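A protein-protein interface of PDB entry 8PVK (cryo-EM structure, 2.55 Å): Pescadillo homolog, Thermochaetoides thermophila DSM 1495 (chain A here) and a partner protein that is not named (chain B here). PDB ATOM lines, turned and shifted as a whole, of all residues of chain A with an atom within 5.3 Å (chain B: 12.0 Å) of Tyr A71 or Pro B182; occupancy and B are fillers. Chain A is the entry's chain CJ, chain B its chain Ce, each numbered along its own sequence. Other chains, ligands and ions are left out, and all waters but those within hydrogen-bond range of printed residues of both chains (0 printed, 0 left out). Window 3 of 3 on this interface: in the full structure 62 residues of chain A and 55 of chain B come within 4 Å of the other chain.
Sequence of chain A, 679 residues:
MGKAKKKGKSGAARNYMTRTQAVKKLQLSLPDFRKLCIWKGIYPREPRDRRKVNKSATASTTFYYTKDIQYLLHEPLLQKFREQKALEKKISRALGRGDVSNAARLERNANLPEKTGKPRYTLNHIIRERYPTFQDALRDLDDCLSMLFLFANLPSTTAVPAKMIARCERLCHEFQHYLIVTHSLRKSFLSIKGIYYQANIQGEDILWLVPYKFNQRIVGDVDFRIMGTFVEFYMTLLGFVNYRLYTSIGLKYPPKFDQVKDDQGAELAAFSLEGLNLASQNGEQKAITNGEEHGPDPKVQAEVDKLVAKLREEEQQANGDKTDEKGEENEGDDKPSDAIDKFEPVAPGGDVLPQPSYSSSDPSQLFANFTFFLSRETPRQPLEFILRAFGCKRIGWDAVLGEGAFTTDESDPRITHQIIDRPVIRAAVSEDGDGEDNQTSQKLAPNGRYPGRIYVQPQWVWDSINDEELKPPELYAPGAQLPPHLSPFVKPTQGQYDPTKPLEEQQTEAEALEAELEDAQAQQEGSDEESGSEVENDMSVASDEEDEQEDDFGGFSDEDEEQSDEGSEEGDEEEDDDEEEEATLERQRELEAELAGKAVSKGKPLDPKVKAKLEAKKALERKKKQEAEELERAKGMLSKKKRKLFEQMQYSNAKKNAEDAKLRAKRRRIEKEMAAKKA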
ATOM      1  N   LYS A  40       4.090  30.792  18.728  1.00  0.00           N
ATOM      2  CA  LYS A  40       3.346  29.543  18.777  1.00  0.00           C
ATOM      3  C   LYS A  40       2.114  29.536  17.882  1.00  0.00           C
ATOM      4  O   LYS A  40       1.426  28.514  17.812  1.00  0.00           O
ATOM      5  CB  LYS A  40       2.936  29.232  20.218  1.00  0.00           C
ATOM      6  CG  LYS A  40       4.111  29.041  21.157  1.00  0.00           C
ATOM      7  CD  LYS A  40       4.562  27.596  21.191  1.00  0.00           C
ATOM      8  CE  LYS A  40       3.549  26.719  21.898  1.00  0.00           C
ATOM      9  NZ  LYS A  40       4.102  25.364  22.166  1.00  0.00           N
ATOM     10  N   THR A  66      -9.571  29.077  24.902  1.00  0.00           N
ATOM     11  CA  THR A  66      -9.170  28.591  26.217  1.00  0.00           C
ATOM     12  C   THR A  66      -8.217  27.410  26.094  1.00  0.00           C
ATOM     13  O   THR A  66      -7.230  27.324  26.830  1.00  0.00           O
ATOM     14  CB  THR A  66     -10.413  28.213  27.025  1.00  0.00           C
ATOM     15  OG1 THR A  66     -11.261  29.360  27.158  1.00  0.00           O
ATOM     16  CG2 THR A  66     -10.041  27.694  28.411  1.00  0.00           C
ATOM     17  N   LYS A  67      -8.476  26.514  25.139  1.00  0.00           N
ATOM     18  CA  LYS A  67      -7.582  25.386  24.904  1.00  0.00           C
ATOM     19  C   LYS A  67      -6.232  25.839  24.355  1.00  0.00           C
ATOM     20  O   LYS A  67      -5.207  25.215  24.648  1.00  0.00           O
ATOM     21  CB  LYS A  67      -8.245  24.394  23.952  1.00  0.00           C
ATOM     22  CG  LYS A  67      -9.548  23.831  24.490  1.00  0.00           C
ATOM     23  CD  LYS A  67      -9.335  23.112  25.811  1.00  0.00           C
ATOM     24  CE  LYS A  67     -10.641  22.556  26.353  1.00  0.00           C
ATOM     25  NZ  LYS A  67     -11.153  21.423  25.536  1.00  0.00           N
ATOM     26  N   ASP A  68      -6.211  26.919  23.567  1.00  0.00           N
ATOM     27  CA  ASP A  68      -4.942  27.480  23.112  1.00  0.00           C
ATOM     28  C   ASP A  68      -4.127  28.031  24.275  1.00  0.00           C
ATOM     29  O   ASP A  68      -2.906  27.836  24.334  1.00  0.00           O
ATOM     30  CB  ASP A  68      -5.192  28.569  22.070  1.00  0.00           C
ATOM     31  CG  ASP A  68      -5.632  28.007  20.736  1.00  0.00           C
ATOM     32  OD1 ASP A  68      -5.700  26.767  20.607  1.00  0.00           O
ATOM     33  OD2 ASP A  68      -5.902  28.803  19.812  1.00  0.00           O
ATOM     34  N   ILE A  69      -4.784  28.713  25.218  1.00  0.00           N
ATOM     35  CA  ILE A  69      -4.067  29.183  26.403  1.00  0.00           C
ATOM     36  C   ILE A  69      -3.615  28.007  27.273  1.00  0.00           C
ATOM     37  O   ILE A  69      -2.530  28.045  27.875  1.00  0.00           O
ATOM     38  CB  ILE A  69      -4.940  30.188  27.178  1.00  0.00           C
ATOM     39  CG1 ILE A  69      -5.369  31.327  26.253  1.00  0.00           C
ATOM     40  CG2 ILE A  69      -4.191  30.764  28.368  1.00  0.00           C
ATOM     41  CD1 ILE A  69      -4.211  32.049  25.591  1.00  0.00           C
ATOM     42  N   GLN A  70      -4.420  26.940  27.335  1.00  0.00           N
ATOM     43  CA  GLN A  70      -4.011  25.728  28.042  1.00  0.00           C
ATOM     44  C   GLN A  70      -2.767  25.112  27.415  1.00  0.00           C
ATOM     45  O   GLN A  70      -1.880  24.626  28.125  1.00  0.00           O
ATOM     46  CB  GLN A  70      -5.149  24.704  28.050  1.00  0.00           C
ATOM     47  CG  GLN A  70      -6.352  25.069  28.903  1.00  0.00           C
ATOM     48  CD  GLN A  70      -5.969  25.613  30.257  1.00  0.00           C
ATOM     49  OE1 GLN A  70      -6.372  26.714  30.632  1.00  0.00           O
ATOM     50  NE2 GLN A  70      -5.200  24.838  31.011  1.00  0.00           N
ATOM     51  N   TYR A  71      -2.700  25.107  26.083  1.00  0.00           N
ATOM     52  CA  TYR A  71      -1.505  24.625  25.398  1.00  0.00           C
ATOM     53  C   TYR A  71      -0.307  25.526  25.676  1.00  0.00           C
ATOM     54  O   TYR A  71       0.818  25.039  25.840  1.00  0.00           O
ATOM     55  CB  TYR A  71      -1.764  24.533  23.897  1.00  0.00           C
ATOM     56  CG  TYR A  71      -0.660  23.840  23.138  1.00  0.00           C
ATOM     57  CD1 TYR A  71      -0.449  22.476  23.278  1.00  0.00           C
ATOM     58  CD2 TYR A  71       0.183  24.552  22.297  1.00  0.00           C
ATOM     59  CE1 TYR A  71       0.561  21.837  22.591  1.00  0.00           C
ATOM     60  CE2 TYR A  71       1.194  23.922  21.602  1.00  0.00           C
ATOM     61  CZ  TYR A  71       1.380  22.565  21.754  1.00  0.00           C
ATOM     62  OH  TYR A  71       2.390  21.933  21.068  1.00  0.00           O
ATOM     63  N   LEU A  72      -0.531  26.843  25.727  1.00  0.00           N
ATOM     64  CA  LEU A  72       0.545  27.778  26.046  1.00  0.00           C
ATOM     65  C   LEU A  72       1.047  27.631  27.476  1.00  0.00           C
ATOM     66  O   LEU A  72       2.181  28.026  27.762  1.00  0.00           O
ATOM     67  CB  LEU A  72       0.081  29.217  25.823  1.00  0.00           C
ATOM     68  CG  LEU A  72       0.159  29.770  24.402  1.00  0.00           C
ATOM     69  CD1 LEU A  72      -0.166  31.253  24.407  1.00  0.00           C
ATOM     70  CD2 LEU A  72       1.529  29.516  23.802  1.00  0.00           C
ATOM     71  N   LEU A  73       0.220  27.095  28.379  1.00  0.00           N
ATOM     72  CA  LEU A  73       0.651  26.879  29.760  1.00  0.00           C
ATOM     73  C   LEU A  73       1.797  25.878  29.884  1.00  0.00           C
ATOM     74  O   LEU A  73       2.517  25.908  30.888  1.00  0.00           O
ATOM     75  CB  LEU A  73      -0.521  26.396  30.613  1.00  0.00           C
ATOM     76  CG  LEU A  73      -1.294  27.448  31.405  1.00  0.00           C
ATOM     77  CD1 LEU A  73      -2.569  26.847  31.959  1.00  0.00           C
ATOM     78  CD2 LEU A  73      -0.433  28.011  32.522  1.00  0.00           C
ATOM     79  N   HIS A  74       1.983  24.994  28.907  1.00  0.00           N
ATOM     80  CA  HIS A  74       2.997  23.949  28.984  1.00  0.00           C
ATOM     81  C   HIS A  74       4.242  24.257  28.161  1.00  0.00           C
ATOM     82  O   HIS A  74       5.089  23.376  27.988  1.00  0.00           O
ATOM     83  CB  HIS A  74       2.405  22.611  28.541  1.00  0.00           C
ATOM     84  CG  HIS A  74       1.327  22.098  29.442  1.00  0.00           C
ATOM     85  ND1 HIS A  74       1.593  21.354  30.571  1.00  0.00           N
ATOM     86  CD2 HIS A  74      -0.020  22.216  29.377  1.00  0.00           C
ATOM     87  CE1 HIS A  74       0.457  21.040  31.166  1.00  0.00           C
ATOM     88  NE2 HIS A  74      -0.537  21.551  30.462  1.00  0.00           N
ATOM     89  N   GLU A  75       4.374  25.474  27.653  1.00  0.00           N
ATOM     90  CA  GLU A  75       5.510  25.811  26.803  1.00  0.00           C
ATOM     91  C   GLU A  75       6.764  25.996  27.653  1.00  0.00           C
ATOM     92  O   GLU A  75       6.731  26.739  28.638  1.00  0.00           O
ATOM     93  CB  GLU A  75       5.217  27.077  26.002  1.00  0.00           C
ATOM     94  CG  GLU A  75       6.423  27.696  25.314  1.00  0.00           C
ATOM     95  CD  GLU A  75       7.039  26.788  24.266  1.00  0.00           C
ATOM     96  OE1 GLU A  75       6.290  26.046  23.597  1.00  0.00           O
ATOM     97  OE2 GLU A  75       8.277  26.815  24.110  1.00  0.00           O
ATOM     98  N   GLU A 129       7.175  22.028  16.076  1.00  0.00           N
ATOM     99  CA  GLU A 129       5.763  22.048  16.449  1.00  0.00           C
ATOM    100  C   GLU A 129       4.913  22.745  15.391  1.00  0.00           C
ATOM    101  O   GLU A 129       3.839  22.253  15.025  1.00  0.00           O
ATOM    102  CB  GLU A 129       5.588  22.726  17.807  1.00  0.00           C
ATOM    103  CG  GLU A 129       4.145  23.048  18.158  1.00  0.00           C
ATOM    104  CD  GLU A 129       4.025  24.190  19.145  1.00  0.00           C
ATOM    105  OE1 GLU A 129       4.923  24.335  20.001  1.00  0.00           O
ATOM    106  OE2 GLU A 129       3.034  24.945  19.062  1.00  0.00           O
ATOM    107  N   PRO B 180       1.160  16.786  33.124  1.00  0.00           N
ATOM    108  CA  PRO B 180       1.194  16.016  31.877  1.00  0.00           C
ATOM    109  C   PRO B 180       1.293  16.907  30.641  1.00  0.00           C
ATOM    110  O   PRO B 180       0.438  17.766  30.427  1.00  0.00           O
ATOM    111  CB  PRO B 180      -0.134  15.256  31.899  1.00  0.00           C
ATOM    112  CG  PRO B 180      -0.462  15.131  33.344  1.00  0.00           C
ATOM    113  CD  PRO B 180       0.028  16.396  33.982  1.00  0.00           C
ATOM    114  N   ASP B 181       2.332  16.697  29.846  1.00  0.00           N
ATOM    115  CA  ASP B 181       2.550  17.519  28.662  1.00  0.00           C
ATOM    116  C   ASP B 181       1.579  17.092  27.564  1.00  0.00           C
ATOM    117  O   ASP B 181       1.491  15.899  27.249  1.00  0.00           O
ATOM    118  CB  ASP B 181       4.008  17.388  28.200  1.00  0.00           C
ATOM    119  CG  ASP B 181       4.396  18.391  27.110  1.00  0.00           C
ATOM    120  OD1 ASP B 181       5.436  19.059  27.286  1.00  0.00           O
ATOM    121  OD2 ASP B 181       3.718  18.492  26.065  1.00  0.00           O
ATOM    122  N   PRO B 182       0.838  18.025  26.962  1.00  0.00           N
ATOM    123  CA  PRO B 182      -0.016  17.672  25.822  1.00  0.00           C
ATOM    124  C   PRO B 182       0.787  17.542  24.539  1.00  0.00           C
ATOM    125  O   PRO B 182       0.945  18.518  23.800  1.00  0.00           O
ATOM    126  CB  PRO B 182      -1.016  18.834  25.751  1.00  0.00           C
ATOM    127  CG  PRO B 182      -0.363  19.974  26.470  1.00  0.00           C
ATOM    128  CD  PRO B 182       0.825  19.469  27.242  1.00  0.00           C
ATOM    129  N   LEU B 183       1.321  16.343  24.287  1.00  0.00           N
ATOM    130  CA  LEU B 183       2.163  16.106  23.118  1.00  0.00           C
ATOM    131  C   LEU B 183       1.422  16.320  21.802  1.00  0.00           C
ATOM    132  O   LEU B 183       2.063  16.590  20.781  1.00  0.00           O
ATOM    133  CB  LEU B 183       2.737  14.688  23.173  1.00  0.00           C
ATOM    134  CG  LEU B 183       4.012  14.410  22.375  1.00  0.00           C
ATOM    135  CD1 LEU B 183       5.162  15.261  22.891  1.00  0.00           C
ATOM    136  CD2 LEU B 183       4.368  12.933  22.431  1.00  0.00           C
ATOM    137  N   LYS B 184       0.097  16.212  21.800  1.00  0.00           N
ATOM    138  CA  LYS B 184      -0.696  16.532  20.624  1.00  0.00           C
ATOM    139  C   LYS B 184      -1.137  17.992  20.665  1.00  0.00           C
ATOM    140  O   LYS B 184      -1.124  18.646  21.711  1.00  0.00           O
ATOM    141  CB  LYS B 184      -1.916  15.614  20.525  1.00  0.00           C
ATOM    142  CG  LYS B 184      -3.089  16.049  21.388  1.00  0.00           C
ATOM    143  CD  LYS B 184      -4.308  15.172  21.172  1.00  0.00           C
ATOM    144  CE  LYS B 184      -5.514  15.728  21.911  1.00  0.00           C
ATOM    145  NZ  LYS B 184      -6.717  14.866  21.746  1.00  0.00           N
ATOM    146  N   LYS B 185      -1.524  18.507  19.493  1.00  0.00           N
ATOM    147  CA  LYS B 185      -2.021  19.873  19.444  1.00  0.00           C
ATOM    148  C   LYS B 185      -3.546  19.887  19.403  1.00  0.00           C
ATOM    149  O   LYS B 185      -4.166  18.987  18.830  1.00  0.00           O
ATOM    150  CB  LYS B 185      -1.471  20.599  18.220  1.00  0.00           C
ATOM    151  CG  LYS B 185       0.037  20.778  18.231  1.00  0.00           C
ATOM    152  CD  LYS B 185       0.540  21.290  16.892  1.00  0.00           C
ATOM    153  CE  LYS B 185      -0.143  22.592  16.507  1.00  0.00           C
ATOM    154  NZ  LYS B 185       0.364  23.121  15.212  1.00  0.00           N
ATOM    155  N   PRO B 186      -4.171  20.890  20.018  1.00  0.00           N
ATOM    156  CA  PRO B 186      -5.636  20.950  20.029  1.00  0.00           C
ATOM    157  C   PRO B 186      -6.220  21.268  18.658  1.00  0.00           C
ATOM    158  O   PRO B 186      -5.600  21.911  17.804  1.00  0.00           O
ATOM    159  CB  PRO B 186      -5.939  22.072  21.029  1.00  0.00           C
ATOM    160  CG  PRO B 186      -4.704  22.204  21.853  1.00  0.00           C
ATOM    161  CD  PRO B 186      -3.575  21.883  20.927  1.00  0.00           C
ATOM    162  N   LYS B 187      -7.458  20.801  18.467  1.00  0.00           N
ATOM    163  CA  LYS B 187      -8.224  21.139  17.275  1.00  0.00           C
ATOM    164  C   LYS B 187      -8.493  22.634  17.174  1.00  0.00           C
ATOM    165  O   LYS B 187      -8.611  23.157  16.061  1.00  0.00           O
ATOM    166  CB  LYS B 187      -9.545  20.368  17.270  1.00  0.00           C
ATOM    167  CG  LYS B 187      -9.391  18.886  17.576  1.00  0.00           C
ATOM    168  CD  LYS B 187     -10.741  18.212  17.750  1.00  0.00           C
ATOM    169  CE  LYS B 187     -11.377  18.597  19.076  1.00  0.00           C
ATOM    170  NZ  LYS B 187     -12.771  18.088  19.194  1.00  0.00           N
ATOM    171  N   THR B 188      -8.575  23.326  18.313  1.00  0.00           N
ATOM    172  CA  THR B 188      -8.660  24.781  18.301  1.00  0.00           C
ATOM    173  C   THR B 188      -7.414  25.406  17.687  1.00  0.00           C
ATOM    174  O   THR B 188      -7.512  26.413  16.977  1.00  0.00           O
ATOM    175  CB  THR B 188      -8.871  25.300  19.723  1.00  0.00           C
ATOM    176  OG1 THR B 188      -7.887  24.730  20.594  1.00  0.00           O
ATOM    177  CG2 THR B 188     -10.255  24.927  20.222  1.00  0.00           C
ATOM    178  N   LEU B 189      -6.239  24.828  17.949  1.00  0.00           N
ATOM    179  CA  LEU B 189      -5.034  25.263  17.254  1.00  0.00           C
ATOM    180  C   LEU B 189      -5.063  24.876  15.783  1.00  0.00           C
ATOM    181  O   LEU B 189      -4.532  25.608  14.940  1.00  0.00           O
ATOM    182  CB  LEU B 189      -3.792  24.677  17.921  1.00  0.00           C
ATOM    183  CG  LEU B 189      -3.066  25.563  18.928  1.00  0.00           C
ATOM    184  CD1 LEU B 189      -1.804  24.871  19.383  1.00  0.00           C
ATOM    185  CD2 LEU B 189      -2.746  26.917  18.322  1.00  0.00           C
ATOM    186  N   GLU B 190      -5.666  23.729  15.454  1.00  0.00           N
ATOM    187  CA  GLU B 190      -5.780  23.330  14.055  1.00  0.00           C
ATOM    188  C   GLU B 190      -6.751  24.200  13.260  1.00  0.00           C
ATOM    189  O   GLU B 190      -6.703  24.179  12.025  1.00  0.00           O
ATOM    190  CB  GLU B 190      -6.207  21.865  13.949  1.00  0.00           C
ATOM    191  CG  GLU B 190      -5.321  20.898  14.716  1.00  0.00           C
ATOM    192  CD  GLU B 190      -5.908  19.501  14.789  1.00  0.00           C
ATOM    193  OE1 GLU B 190      -7.036  19.302  14.292  1.00  0.00           O
ATOM    194  OE2 GLU B 190      -5.240  18.602  15.343  1.00  0.00           O
ATOM    195  N   GLN B 191      -7.641  24.928  13.936  1.00  0.00           N
ATOM    196  CA  GLN B 191      -8.535  25.860  13.251  1.00  0.00           C
ATOM    197  C   GLN B 191      -7.750  26.948  12.524  1.00  0.00           C
ATOM    198  O   GLN B 191      -6.721  27.428  13.007  1.00  0.00           O
ATOM    199  CB  GLN B 191      -9.504  26.513  14.239  1.00  0.00           C
ATOM    200  CG  GLN B 191     -10.413  25.558  14.983  1.00  0.00           C
ATOM    201  CD  GLN B 191     -11.677  25.243  14.216  1.00  0.00           C
ATOM    202  OE1 GLN B 191     -12.174  26.068  13.450  1.00  0.00           O
ATOM    203  NE2 GLN B 191     -12.206  24.042  14.414  1.00  0.00           N
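Thr A66 touches none of the printed residues of chain B. Of the printed residues of chain B, Asp A68 touches Thr B188 (3.0 Å) and Leu B189 (3.3 Å). No residue of chain B comes within 4 Å of Ile A69. Tyr A71 touches just these residues of chain B: Pro B182 (3.6 Å), Lys B184 (3.7 Å), Lys B185 (3.9 Å), Pro B186 (3.96 Å) and Leu B189 (3.5 Å). No residue of chain B comes within 4 Å of Leu A72. No residue of chain B comes within 4 Å of Leu A73. Of the printed residues of chain B, His A74 touches Pro B180 (3.4 Å) and Pro B182 (3.5 Å). No residue of chain B comes within 4 Å of Glu A75. Of chain B, only Lys B185 (3.6 Å) comes within 4 Å of Glu A129. Of the printed residues of chain A, Pro B180 touches His A74 (3.4 Å). Pro B182 touches just these residues of chain A: Tyr A71 and His A74. Of the printed residues of chain A, Thr B188 touches Lys A67 and Asp A68. The nearest residue of chain B that does not touch Tyr A71 is Leu B183 (5.4 Å).
Of the 12 printed residues of chain A, 5 touch a printed residue of chain B. Among the printed residues, no Asp or Glu carboxylate lies within 4 Å of a Lys or Arg side-chain nitrogen of the other chain.
Lys A67 touches Thr B188 (CB to OG1, 3.4 Å). CE1 of Tyr A71 touches O of Pro B182 (3.6 Å). CE1 of Tyr A71 touches O of Lys B184, at 3.7 Å. OH of Tyr A71 touches CG of Lys B185, 3.9 Å away. CD of Pro B186 touches CD1 of Tyr A71, at 3.96 Å. Tyr A71 touches Leu B189 (CD2 to CD1, 3.5 Å). Pro B180 touches His A74. CG of His A74 touches CD of Pro B182 (3.5 Å). O of Glu A129 touches NZ of Lys B185, at 3.6 Å.
The side-chain hydroxyl of Thr B188 lies within hydrogen-bond range of the side-chain carboxylate of Asp A68 (3.0 Å). N of Leu B189 lies within hydrogen-bond range of OD1 of Asp A68, 3.3 Å away.
The side-chain amino group (NZ) of Lys A40 lies within salt-bridge range of the side-chain carboxylate (OE1) of Glu A129 (2.5 Å).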
